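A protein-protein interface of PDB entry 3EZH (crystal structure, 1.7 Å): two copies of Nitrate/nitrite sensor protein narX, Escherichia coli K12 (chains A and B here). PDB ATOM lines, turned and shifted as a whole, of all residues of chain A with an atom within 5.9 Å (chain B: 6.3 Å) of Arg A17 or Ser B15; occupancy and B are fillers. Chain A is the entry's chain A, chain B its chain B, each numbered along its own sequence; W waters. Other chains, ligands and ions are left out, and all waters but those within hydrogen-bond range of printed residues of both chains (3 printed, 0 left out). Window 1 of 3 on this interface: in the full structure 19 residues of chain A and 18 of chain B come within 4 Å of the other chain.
The side-chain amide oxygen (OD1) of Asn B11 sits at hydrogen-bond distance from the guanidinium group (NH1) of Arg A17, at 2.9 Å.
The guanidinium group (NH1) of Arg A22 sits at hydrogen-bond distance from the side-chain sulfur (SD) of Met A18 (3.7 Å).
The side-chain carboxylate of Asp A98 is in salt-bridge range of the guanidinium group of Arg A17, at 3.0 Å.
NE of Arg A17 sits close to O of Gly A14.
OG of Ser B15 sits at hydrogen-bond distance from NE2 of Gln B19, at 3.2 Å.
The backbone carbonyl oxygen of Lys B12 sits at hydrogen-bond distance from the side-chain hydroxyl of Ser B15, at 2.7 Å.
The backbone carbonyl oxygen of Gly B14 lies close to the guanidinium group of Arg B17.
Among the printed residues, pairs that only touch across the chains: Arg A22 with Tyr B21 (3.4 Å), Val A101 with Asn B11 (3.5 Å), Met A18 with Tyr B21 (3.6 Å), Ser A15 with Arg B17 (3.6 Å), Arg A17 with Ser B15 (3.7 Å), Tyr A21 with Tyr B21 (3.7 Å), Tyr A21 with Met B18 (3.7 Å), Arg A17 with Met B18 (3.8 Å), Met A18 with Arg B17 (3.8 Å), Met A18 with Met B18 (3.8 Å), Ile A10 with Ile B10 (3.9 Å), Val A94 with Met B18 (3.9 Å) and Ile A10 with Asn B11 (3.97 Å).
Of the printed residues of chain B, Ile A10 touches Ile B10 and Asn B11.
Ser A20 touches none of the printed residues of chain B.
Printed residues of chain B within 4 Å of Arg A22: Tyr B21 (3.4 Å).
Of the printed residues of chain A, Ile B10 touches Ile A10.
Ser B15 touches one residue of chain A.
The nearest residue of chain B that does not touch Arg A17 is Gly B14 (4.1 Å).
The nearest residue of chain A that does not touch Ser B15 is Asp A98 (5.8 Å).
Of the 16 printed residues of chain A, 8 touch a printed residue of chain B.
Hydrophobic or aromatic side chains of chain A within 4 Å of the printed part of chain B: Ile A10, Met A18, Tyr A21, Val A94 and Val A101.
Printed residues of chain B that touch a printed residue of chain A: Ile B10, Asn B11, Ser B15, Arg B17, Met B18 and Tyr B21.
Hydrophobic or aromatic side chains of chain B within 4 Å of the printed part of chain A: Ile B10, Met B18 and Tyr B21.
Among the printed residues, no Asp or Glu carboxylate lies within 4 Å of a Lys or Arg side-chain nitrogen of the other chain.
Ser A15 touches Arg B17, and with the chains exchanged Arg A17 touches Ser B15.
Arg A17 touches Met B18, and with the chains exchanged Met A18 touches Arg B17.
Met B18 touches its own counterpart, Met A18.
Tyr B21 touches its own counterpart, Tyr A21.
Of the 14 pairs that touch across the chains among the printed residues, 9 have their exchanged pair printed and touching as well.
Water W3 lies within hydrogen-bond range of the side-chain hydroxyl (OH) of Tyr B21 and the guanidinium group (NH1) of Arg A22.
Water W2 lies within hydrogen-bond range of the side-chain amide nitrogen of Asn B11 (2.9 Å), the backbone carbonyl oxygen of Asp A98 (2.9 Å) and the guanidinium group of Arg A17 (3.4 Å).
Water W1 lies within hydrogen-bond range of O of Ile B10, O of Ile A10 and NH2 of Arg B17.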
ATOM      1  N   ILE A  10     -27.601 -33.539   2.582  1.00  0.00           N
ATOM      2  CA  ILE A  10     -26.437 -33.154   1.724  1.00  0.00           C
ATOM      3  C   ILE A  10     -25.973 -31.764   2.209  1.00  0.00           C
ATOM      4  O   ILE A  10     -24.800 -31.509   2.346  1.00  0.00           O
ATOM      5  CB  ILE A  10     -26.808 -33.121   0.227  1.00  0.00           C
ATOM      6  CG1 ILE A  10     -27.190 -34.539  -0.202  1.00  0.00           C
ATOM      7  CG2 ILE A  10     -25.648 -32.641  -0.711  1.00  0.00           C
ATOM      8  CD1 ILE A  10     -27.577 -34.650  -1.648  1.00  0.00           C
ATOM      9  N   ALA A  13     -24.244 -32.261   5.732  1.00  0.00           N
ATOM     10  CA  ALA A  13     -22.937 -32.947   5.620  1.00  0.00           C
ATOM     11  C   ALA A  13     -21.933 -32.015   4.927  1.00  0.00           C
ATOM     12  O   ALA A  13     -20.759 -31.914   5.337  1.00  0.00           O
ATOM     13  CB  ALA A  13     -23.101 -34.229   4.802  1.00  0.00           C
ATOM     14  N   GLY A  14     -22.367 -31.372   3.840  1.00  0.00           N
ATOM     15  CA  GLY A  14     -21.447 -30.431   3.193  1.00  0.00           C
ATOM     16  C   GLY A  14     -21.021 -29.341   4.146  1.00  0.00           C
ATOM     17  O   GLY A  14     -19.877 -28.886   4.134  1.00  0.00           O
ATOM     18  N   SER A  15     -21.928 -28.887   5.007  1.00  0.00           N
ATOM     19  CA  SER A  15     -21.542 -27.817   5.910  1.00  0.00           C
ATOM     20  C   SER A  15     -20.385 -28.160   6.831  1.00  0.00           C
ATOM     21  O   SER A  15     -19.748 -27.262   7.357  1.00  0.00           O
ATOM     22  CB  SER A  15     -22.740 -27.316   6.738  1.00  0.00           C
ATOM     23  OG  SER A  15     -22.968 -28.113   7.920  1.00  0.00           O
ATOM     24  N   LEU A  16     -20.137 -29.450   7.078  1.00  0.00           N
ATOM     25  CA  LEU A  16     -18.992 -29.798   7.890  1.00  0.00           C
ATOM     26  C   LEU A  16     -17.672 -29.320   7.239  1.00  0.00           C
ATOM     27  O   LEU A  16     -16.683 -29.137   7.944  1.00  0.00           O
ATOM     28  CB  LEU A  16     -18.905 -31.342   8.044  1.00  0.00           C
ATOM     29  CG  LEU A  16     -20.071 -31.860   8.914  1.00  0.00           C
ATOM     30  CD1 LEU A  16     -20.118 -33.413   8.778  1.00  0.00           C
ATOM     31  CD2 LEU A  16     -19.882 -31.477  10.405  1.00  0.00           C
ATOM     32  N   ARG A  17     -17.668 -29.168   5.912  1.00  0.00           N
ATOM     33  CA  ARG A  17     -16.452 -28.717   5.231  1.00  0.00           C
ATOM     34  C   ARG A  17     -16.241 -27.270   5.586  1.00  0.00           C
ATOM     35  O   ARG A  17     -15.157 -26.838   5.931  1.00  0.00           O
ATOM     36  CB  ARG A  17     -16.626 -28.862   3.717  1.00  0.00           C
ATOM     37  CG  ARG A  17     -16.936 -30.332   3.275  1.00  0.00           C
ATOM     38  CD  ARG A  17     -17.095 -30.392   1.792  1.00  0.00           C
ATOM     39  NE  ARG A  17     -18.331 -29.741   1.337  1.00  0.00           N
ATOM     40  CZ  ARG A  17     -18.969 -30.018   0.199  1.00  0.00           C
ATOM     41  NH1 ARG A  17     -18.507 -30.954  -0.667  1.00  0.00           N
ATOM     42  NH2 ARG A  17     -20.102 -29.353  -0.057  1.00  0.00           N
ATOM     43  N   MET A  18     -17.311 -26.485   5.465  1.00  0.00           N
ATOM     44  CA  MET A  18     -17.173 -25.106   5.868  1.00  0.00           C
ATOM     45  C   MET A  18     -16.782 -25.003   7.349  1.00  0.00           C
ATOM     46  O   MET A  18     -15.947 -24.157   7.719  1.00  0.00           O
ATOM     47  CB  MET A  18     -18.529 -24.368   5.681  1.00  0.00           C
ATOM     48  CG  MET A  18     -18.485 -22.886   6.108  1.00  0.00           C
ATOM     49  SD  MET A  18     -18.992 -22.618   8.014  1.00  0.00           S
ATOM     50  CE  MET A  18     -20.881 -22.880   7.854  1.00  0.00           C
ATOM     51  N   GLN A  19     -17.365 -25.865   8.211  1.00  0.00           N
ATOM     52  CA  GLN A  19     -17.081 -25.716   9.617  1.00  0.00           C
ATOM     53  C   GLN A  19     -15.656 -26.035   9.961  1.00  0.00           C
ATOM     54  O   GLN A  19     -15.103 -25.480  10.944  1.00  0.00           O
ATOM     55  CB  GLN A  19     -18.078 -26.533  10.440  1.00  0.00           C
ATOM     56  CG  GLN A  19     -19.530 -26.086  10.300  1.00  0.00           C
ATOM     57  CD  GLN A  19     -20.455 -26.939  11.191  1.00  0.00           C
ATOM     58  OE1 GLN A  19     -20.248 -27.016  12.395  1.00  0.00           O
ATOM     59  NE2 GLN A  19     -21.430 -27.631  10.571  1.00  0.00           N
ATOM     60  N   SER A  20     -15.080 -26.937   9.128  1.00  0.00           N
ATOM     61  CA  SER A  20     -13.680 -27.300   9.292  1.00  0.00           C
ATOM     62  C   SER A  20     -12.752 -26.114   9.021  1.00  0.00           C
ATOM     63  O   SER A  20     -11.827 -25.835   9.823  1.00  0.00           O
ATOM     64  CB  SER A  20     -13.295 -28.467   8.330  1.00  0.00           C
ATOM     65  OG  SER A  20     -14.011 -29.642   8.686  1.00  0.00           O
ATOM     66  N   TYR A  21     -12.993 -25.408   7.911  1.00  0.00           N
ATOM     67  CA  TYR A  21     -12.136 -24.294   7.569  1.00  0.00           C
ATOM     68  C   TYR A  21     -12.478 -23.089   8.435  1.00  0.00           C
ATOM     69  O   TYR A  21     -11.617 -22.234   8.653  1.00  0.00           O
ATOM     70  CB  TYR A  21     -12.232 -23.929   6.090  1.00  0.00           C
ATOM     71  CG  TYR A  21     -11.115 -24.626   5.252  1.00  0.00           C
ATOM     72  CD1 TYR A  21      -9.806 -24.197   5.375  1.00  0.00           C
ATOM     73  CD2 TYR A  21     -11.396 -25.700   4.430  1.00  0.00           C
ATOM     74  CE1 TYR A  21      -8.773 -24.856   4.671  1.00  0.00           C
ATOM     75  CE2 TYR A  21     -10.367 -26.364   3.738  1.00  0.00           C
ATOM     76  CZ  TYR A  21      -9.091 -25.929   3.884  1.00  0.00           C
ATOM     77  OH  TYR A  21      -8.044 -26.591   3.203  1.00  0.00           O
ATOM     78  N   ARG A  22     -13.717 -23.012   8.887  1.00  0.00           N
ATOM     79  CA  ARG A  22     -14.018 -21.911   9.824  1.00  0.00           C
ATOM     80  C   ARG A  22     -13.214 -22.083  11.113  1.00  0.00           C
ATOM     81  O   ARG A  22     -12.752 -21.073  11.675  1.00  0.00           O
ATOM     82  CB  ARG A  22     -15.551 -21.856  10.134  1.00  0.00           C
ATOM     83  CG  ARG A  22     -15.907 -20.774  11.207  1.00  0.00           C
ATOM     84  CD  ARG A  22     -17.472 -20.575  11.105  1.00  0.00           C
ATOM     85  NE  ARG A  22     -18.159 -21.698  11.712  1.00  0.00           N
ATOM     86  CZ  ARG A  22     -19.489 -21.883  11.713  1.00  0.00           C
ATOM     87  NH1 ARG A  22     -20.302 -21.012  11.097  1.00  0.00           N
ATOM     88  NH2 ARG A  22     -20.017 -22.931  12.392  1.00  0.00           N
ATOM     89  N   MET A  40     -20.182 -28.248  15.533  1.00  0.00           N
ATOM     90  CA  MET A  40     -19.666 -29.232  14.566  1.00  0.00           C
ATOM     91  C   MET A  40     -19.879 -30.675  15.086  1.00  0.00           C
ATOM     92  O   MET A  40     -20.229 -31.609  14.343  1.00  0.00           O
ATOM     93  CB  MET A  40     -18.161 -28.968  14.238  1.00  0.00           C
ATOM     94  CG  MET A  40     -17.836 -29.511  12.894  1.00  0.00           C
ATOM     95  SD  MET A  40     -15.982 -29.135  12.560  1.00  0.00           S
ATOM     96  CE  MET A  40     -15.769 -30.538  11.215  1.00  0.00           C
ATOM     97  N   VAL A  94     -11.439 -32.130   4.746  1.00  0.00           N
ATOM     98  CA  VAL A  94     -12.425 -31.621   3.811  1.00  0.00           C
ATOM     99  C   VAL A  94     -12.419 -32.490   2.543  1.00  0.00           C
ATOM    100  O   VAL A  94     -13.448 -32.699   1.947  1.00  0.00           O
ATOM    101  CB  VAL A  94     -12.100 -30.173   3.493  1.00  0.00           C
ATOM    102  CG1 VAL A  94     -12.881 -29.695   2.280  1.00  0.00           C
ATOM    103  CG2 VAL A  94     -12.392 -29.382   4.771  1.00  0.00           C
ATOM    104  N   LEU A  97     -14.443 -35.404   3.452  1.00  0.00           N
ATOM    105  CA  LEU A  97     -15.877 -35.008   3.471  1.00  0.00           C
ATOM    106  C   LEU A  97     -16.406 -34.891   2.060  1.00  0.00           C
ATOM    107  O   LEU A  97     -17.569 -35.202   1.825  1.00  0.00           O
ATOM    108  CB  LEU A  97     -16.067 -33.652   4.185  1.00  0.00           C
ATOM    109  CG  LEU A  97     -15.936 -33.783   5.725  1.00  0.00           C
ATOM    110  CD1 LEU A  97     -15.683 -32.327   6.340  1.00  0.00           C
ATOM    111  CD2 LEU A  97     -17.171 -34.433   6.293  1.00  0.00           C
ATOM    112  N   ASP A  98     -15.590 -34.412   1.111  1.00  0.00           N
ATOM    113  CA  ASP A  98     -15.997 -34.256  -0.284  1.00  0.00           C
ATOM    114  C   ASP A  98     -16.397 -35.648  -0.803  1.00  0.00           C
ATOM    115  O   ASP A  98     -17.378 -35.786  -1.521  1.00  0.00           O
ATOM    116  CB  ASP A  98     -14.851 -33.795  -1.222  1.00  0.00           C
ATOM    117  CG  ASP A  98     -14.661 -32.300  -1.270  1.00  0.00           C
ATOM    118  OD1 ASP A  98     -15.577 -31.545  -0.890  1.00  0.00           O
ATOM    119  OD2 ASP A  98     -13.576 -31.870  -1.743  1.00  0.00           O
ATOM    120  N   VAL A 101     -19.845 -36.589   0.766  1.00  0.00           N
ATOM    121  CA  VAL A 101     -20.961 -35.824   0.178  1.00  0.00           C
ATOM    122  C   VAL A 101     -21.208 -36.262  -1.267  1.00  0.00           C
ATOM    123  O   VAL A 101     -22.359 -36.339  -1.686  1.00  0.00           O
ATOM    124  CB  VAL A 101     -20.690 -34.288   0.326  1.00  0.00           C
ATOM    125  CG1 VAL A 101     -21.872 -33.489  -0.288  1.00  0.00           C
ATOM    126  CG2 VAL A 101     -20.561 -33.915   1.794  1.00  0.00           C
ATOM    127  N   ILE B  10     -26.858 -28.757  -4.532  1.00  0.00           N
ATOM    128  CA  ILE B  10     -26.811 -28.434  -3.101  1.00  0.00           C
ATOM    129  C   ILE B  10     -25.340 -28.652  -2.631  1.00  0.00           C
ATOM    130  O   ILE B  10     -24.819 -27.893  -1.823  1.00  0.00           O
ATOM    131  CB  ILE B  10     -27.743 -29.345  -2.291  1.00  0.00           C
ATOM    132  CG1 ILE B  10     -29.195 -29.050  -2.705  1.00  0.00           C
ATOM    133  CG2 ILE B  10     -27.498 -29.201  -0.798  1.00  0.00           C
ATOM    134  CD1 ILE B  10     -30.173 -29.992  -2.043  1.00  0.00           C
ATOM    135  N   ASN B  11     -24.691 -29.676  -3.179  1.00  0.00           N
ATOM    136  CA  ASN B  11     -23.268 -29.969  -2.844  1.00  0.00           C
ATOM    137  C   ASN B  11     -22.365 -28.843  -3.359  1.00  0.00           C
ATOM    138  O   ASN B  11     -21.569 -28.275  -2.626  1.00  0.00           O
ATOM    139  CB  ASN B  11     -22.857 -31.322  -3.513  1.00  0.00           C
ATOM    140  CG  ASN B  11     -21.399 -31.707  -3.252  1.00  0.00           C
ATOM    141  OD1 ASN B  11     -20.684 -31.007  -2.542  1.00  0.00           O
ATOM    142  ND2 ASN B  11     -20.947 -32.825  -3.853  1.00  0.00           N
ATOM    143  N   LYS B  12     -22.537 -28.477  -4.627  1.00  0.00           N
ATOM    144  CA  LYS B  12     -21.695 -27.467  -5.266  1.00  0.00           C
ATOM    145  C   LYS B  12     -21.892 -26.054  -4.699  1.00  0.00           C
ATOM    146  O   LYS B  12     -20.942 -25.336  -4.405  1.00  0.00           O
ATOM    147  CB  LYS B  12     -21.958 -27.518  -6.761  1.00  0.00           C
ATOM    148  CG  LYS B  12     -21.236 -28.632  -7.460  1.00  0.00           C
ATOM    149  CD  LYS B  12     -19.745 -28.443  -7.320  1.00  0.00           C
ATOM    150  CE  LYS B  12     -19.060 -29.754  -6.976  1.00  0.00           C
ATOM    151  NZ  LYS B  12     -17.601 -29.518  -6.745  1.00  0.00           N
ATOM    152  N   ALA B  13     -23.153 -25.666  -4.495  1.00  0.00           N
ATOM    153  CA  ALA B  13     -23.409 -24.338  -3.873  1.00  0.00           C
ATOM    154  C   ALA B  13     -22.852 -24.360  -2.444  1.00  0.00           C
ATOM    155  O   ALA B  13     -22.246 -23.408  -1.966  1.00  0.00           O
ATOM    156  CB  ALA B  13     -24.944 -24.073  -3.814  1.00  0.00           C
ATOM    157  N   GLY B  14     -23.063 -25.479  -1.754  1.00  0.00           N
ATOM    158  CA  GLY B  14     -22.560 -25.587  -0.398  1.00  0.00           C
ATOM    159  C   GLY B  14     -21.046 -25.423  -0.404  1.00  0.00           C
ATOM    160  O   GLY B  14     -20.487 -24.825   0.489  1.00  0.00           O
ATOM    161  N   SER B  15     -20.376 -25.973  -1.409  1.00  0.00           N
ATOM    162  CA  SER B  15     -18.922 -25.873  -1.403  1.00  0.00           C
ATOM    163  C   SER B  15     -18.396 -24.458  -1.410  1.00  0.00           C
ATOM    164  O   SER B  15     -17.281 -24.194  -0.991  1.00  0.00           O
ATOM    165  CB  SER B  15     -18.310 -26.686  -2.592  1.00  0.00           C
ATOM    166  OG  SER B  15     -18.405 -25.971  -3.852  1.00  0.00           O
ATOM    167  N   LEU B  16     -19.164 -23.519  -1.961  1.00  0.00           N
ATOM    168  CA  LEU B  16     -18.721 -22.132  -1.924  1.00  0.00           C
ATOM    169  C   LEU B  16     -18.524 -21.659  -0.487  1.00  0.00           C
ATOM    170  O   LEU B  16     -17.679 -20.755  -0.227  1.00  0.00           O
ATOM    171  CB  LEU B  16     -19.788 -21.259  -2.681  1.00  0.00           C
ATOM    172  CG  LEU B  16     -19.839 -21.537  -4.193  1.00  0.00           C
ATOM    173  CD1 LEU B  16     -21.149 -20.837  -4.734  1.00  0.00           C
ATOM    174  CD2 LEU B  16     -18.553 -20.937  -4.947  1.00  0.00           C
ATOM    175  N   ARG B  17     -19.268 -22.265   0.474  1.00  0.00           N
ATOM    176  CA  ARG B  17     -19.120 -21.843   1.859  1.00  0.00           C
ATOM    177  C   ARG B  17     -17.734 -22.243   2.335  1.00  0.00           C
ATOM    178  O   ARG B  17     -16.997 -21.450   2.918  1.00  0.00           O
ATOM    179  CB  ARG B  17     -20.180 -22.485   2.767  1.00  0.00           C
ATOM    180  CG  ARG B  17     -21.624 -22.074   2.359  1.00  0.00           C
ATOM    181  CD  ARG B  17     -22.696 -22.740   3.255  1.00  0.00           C
ATOM    182  NE  ARG B  17     -22.702 -24.215   3.096  1.00  0.00           N
ATOM    183  CZ  ARG B  17     -23.763 -24.984   3.347  1.00  0.00           C
ATOM    184  NH1 ARG B  17     -24.930 -24.428   3.797  1.00  0.00           N
ATOM    185  NH2 ARG B  17     -23.671 -26.304   3.110  1.00  0.00           N
ATOM    186  N   MET B  18     -17.367 -23.504   2.055  1.00  0.00           N
ATOM    187  CA  MET B  18     -16.040 -23.966   2.431  1.00  0.00           C
ATOM    188  C   MET B  18     -14.946 -23.141   1.695  1.00  0.00           C
ATOM    189  O   MET B  18     -13.990 -22.735   2.345  1.00  0.00           O
ATOM    190  CB  MET B  18     -15.902 -25.479   2.061  1.00  0.00           C
ATOM    191  CG  MET B  18     -14.469 -26.082   2.318  1.00  0.00           C
ATOM    192  SD  MET B  18     -13.130 -25.737   0.833  1.00  0.00           S
ATOM    193  CE  MET B  18     -13.885 -26.910  -0.422  1.00  0.00           C
ATOM    194  N   GLN B  19     -15.125 -22.879   0.389  1.00  0.00           N
ATOM    195  CA  GLN B  19     -14.133 -22.148  -0.409  1.00  0.00           C
ATOM    196  C   GLN B  19     -13.921 -20.748   0.164  1.00  0.00           C
ATOM    197  O   GLN B  19     -12.813 -20.191   0.134  1.00  0.00           O
ATOM    198  CB  GLN B  19     -14.558 -22.150  -1.865  1.00  0.00           C
ATOM    199  CG  GLN B  19     -14.530 -23.578  -2.485  1.00  0.00           C
ATOM    200  CD  GLN B  19     -14.766 -23.519  -3.984  1.00  0.00           C
ATOM    201  OE1 GLN B  19     -13.995 -22.928  -4.671  1.00  0.00           O
ATOM    202  NE2 GLN B  19     -15.852 -24.094  -4.467  1.00  0.00           N
ATOM    203  N   SER B  20     -15.011 -20.148   0.662  1.00  0.00           N
ATOM    204  CA  SER B  20     -14.839 -18.822   1.278  1.00  0.00           C
ATOM    205  C   SER B  20     -13.924 -18.822   2.514  1.00  0.00           C
ATOM    206  O   SER B  20     -13.050 -17.982   2.679  1.00  0.00           O
ATOM    207  CB  SER B  20     -16.233 -18.273   1.677  1.00  0.00           C
ATOM    208  OG  SER B  20     -16.985 -18.091   0.505  1.00  0.00           O
ATOM    209  N   TYR B  21     -14.101 -19.802   3.401  1.00  0.00           N
ATOM    210  CA  TYR B  21     -13.305 -19.847   4.594  1.00  0.00           C
ATOM    211  C   TYR B  21     -11.905 -20.374   4.333  1.00  0.00           C
ATOM    212  O   TYR B  21     -11.005 -20.118   5.152  1.00  0.00           O
ATOM    213  CB  TYR B  21     -13.999 -20.717   5.639  1.00  0.00           C
ATOM    214  CG  TYR B  21     -14.928 -19.909   6.540  1.00  0.00           C
ATOM    215  CD1 TYR B  21     -14.386 -19.097   7.517  1.00  0.00           C
ATOM    216  CD2 TYR B  21     -16.307 -19.999   6.398  1.00  0.00           C
ATOM    217  CE1 TYR B  21     -15.201 -18.347   8.377  1.00  0.00           C
ATOM    218  CE2 TYR B  21     -17.173 -19.242   7.283  1.00  0.00           C
ATOM    219  CZ  TYR B  21     -16.572 -18.437   8.253  1.00  0.00           C
ATOM    220  OH  TYR B  21     -17.365 -17.740   9.171  1.00  0.00           O
ATOM    221  N   THR B  43     -16.744 -22.422  -9.800  1.00  0.00           N
ATOM    222  CA  THR B  43     -17.919 -22.932  -9.114  1.00  0.00           C
ATOM    223  C   THR B  43     -19.100 -21.922  -9.126  1.00  0.00           C
ATOM    224  O   THR B  43     -20.248 -22.268  -9.451  1.00  0.00           O
ATOM    225  CB  THR B  43     -17.608 -23.226  -7.639  1.00  0.00           C
ATOM    226  OG1 THR B  43     -16.448 -24.121  -7.582  1.00  0.00           O
ATOM    227  CG2 THR B  43     -18.814 -23.922  -6.984  1.00  0.00           C
ATOM    228  N   LEU B  97     -24.683 -17.287   1.245  1.00  0.00           N
ATOM    229  CA  LEU B  97     -24.684 -18.599   0.615  1.00  0.00           C
ATOM    230  C   LEU B  97     -25.575 -19.600   1.340  1.00  0.00           C
ATOM    231  O   LEU B  97     -26.192 -20.438   0.666  1.00  0.00           O
ATOM    232  CB  LEU B  97     -23.242 -19.174   0.547  1.00  0.00           C
ATOM    233  CG  LEU B  97     -22.262 -18.420  -0.309  1.00  0.00           C
ATOM    234  CD1 LEU B  97     -20.814 -18.943   0.026  1.00  0.00           C
ATOM    235  CD2 LEU B  97     -22.571 -18.671  -1.779  1.00  0.00           C
ATOM    236  N   VAL B 101     -28.178 -22.097  -0.510  1.00  0.00           N
ATOM    237  CA  VAL B 101     -28.267 -23.550  -0.300  1.00  0.00           C
ATOM    238  C   VAL B 101     -29.571 -24.001   0.316  1.00  0.00           C
ATOM    239  O   VAL B 101     -30.148 -25.027  -0.126  1.00  0.00           O
ATOM    240  CB  VAL B 101     -27.072 -24.097   0.517  1.00  0.00           C
ATOM    241  CG1 VAL B 101     -27.061 -25.638   0.489  1.00  0.00           C
ATOM    242  CG2 VAL B 101     -25.797 -23.633  -0.127  1.00  0.00           C
HETATM  243  O   HOH W   1     -23.691 -28.857   0.832  1.00  0.00           O
HETATM  244  O   HOH W   2     -18.218 -33.387  -3.008  1.00  0.00           O
HETATM  245  O   HOH W   3     -19.715 -18.368  10.066  1.00  0.00           O
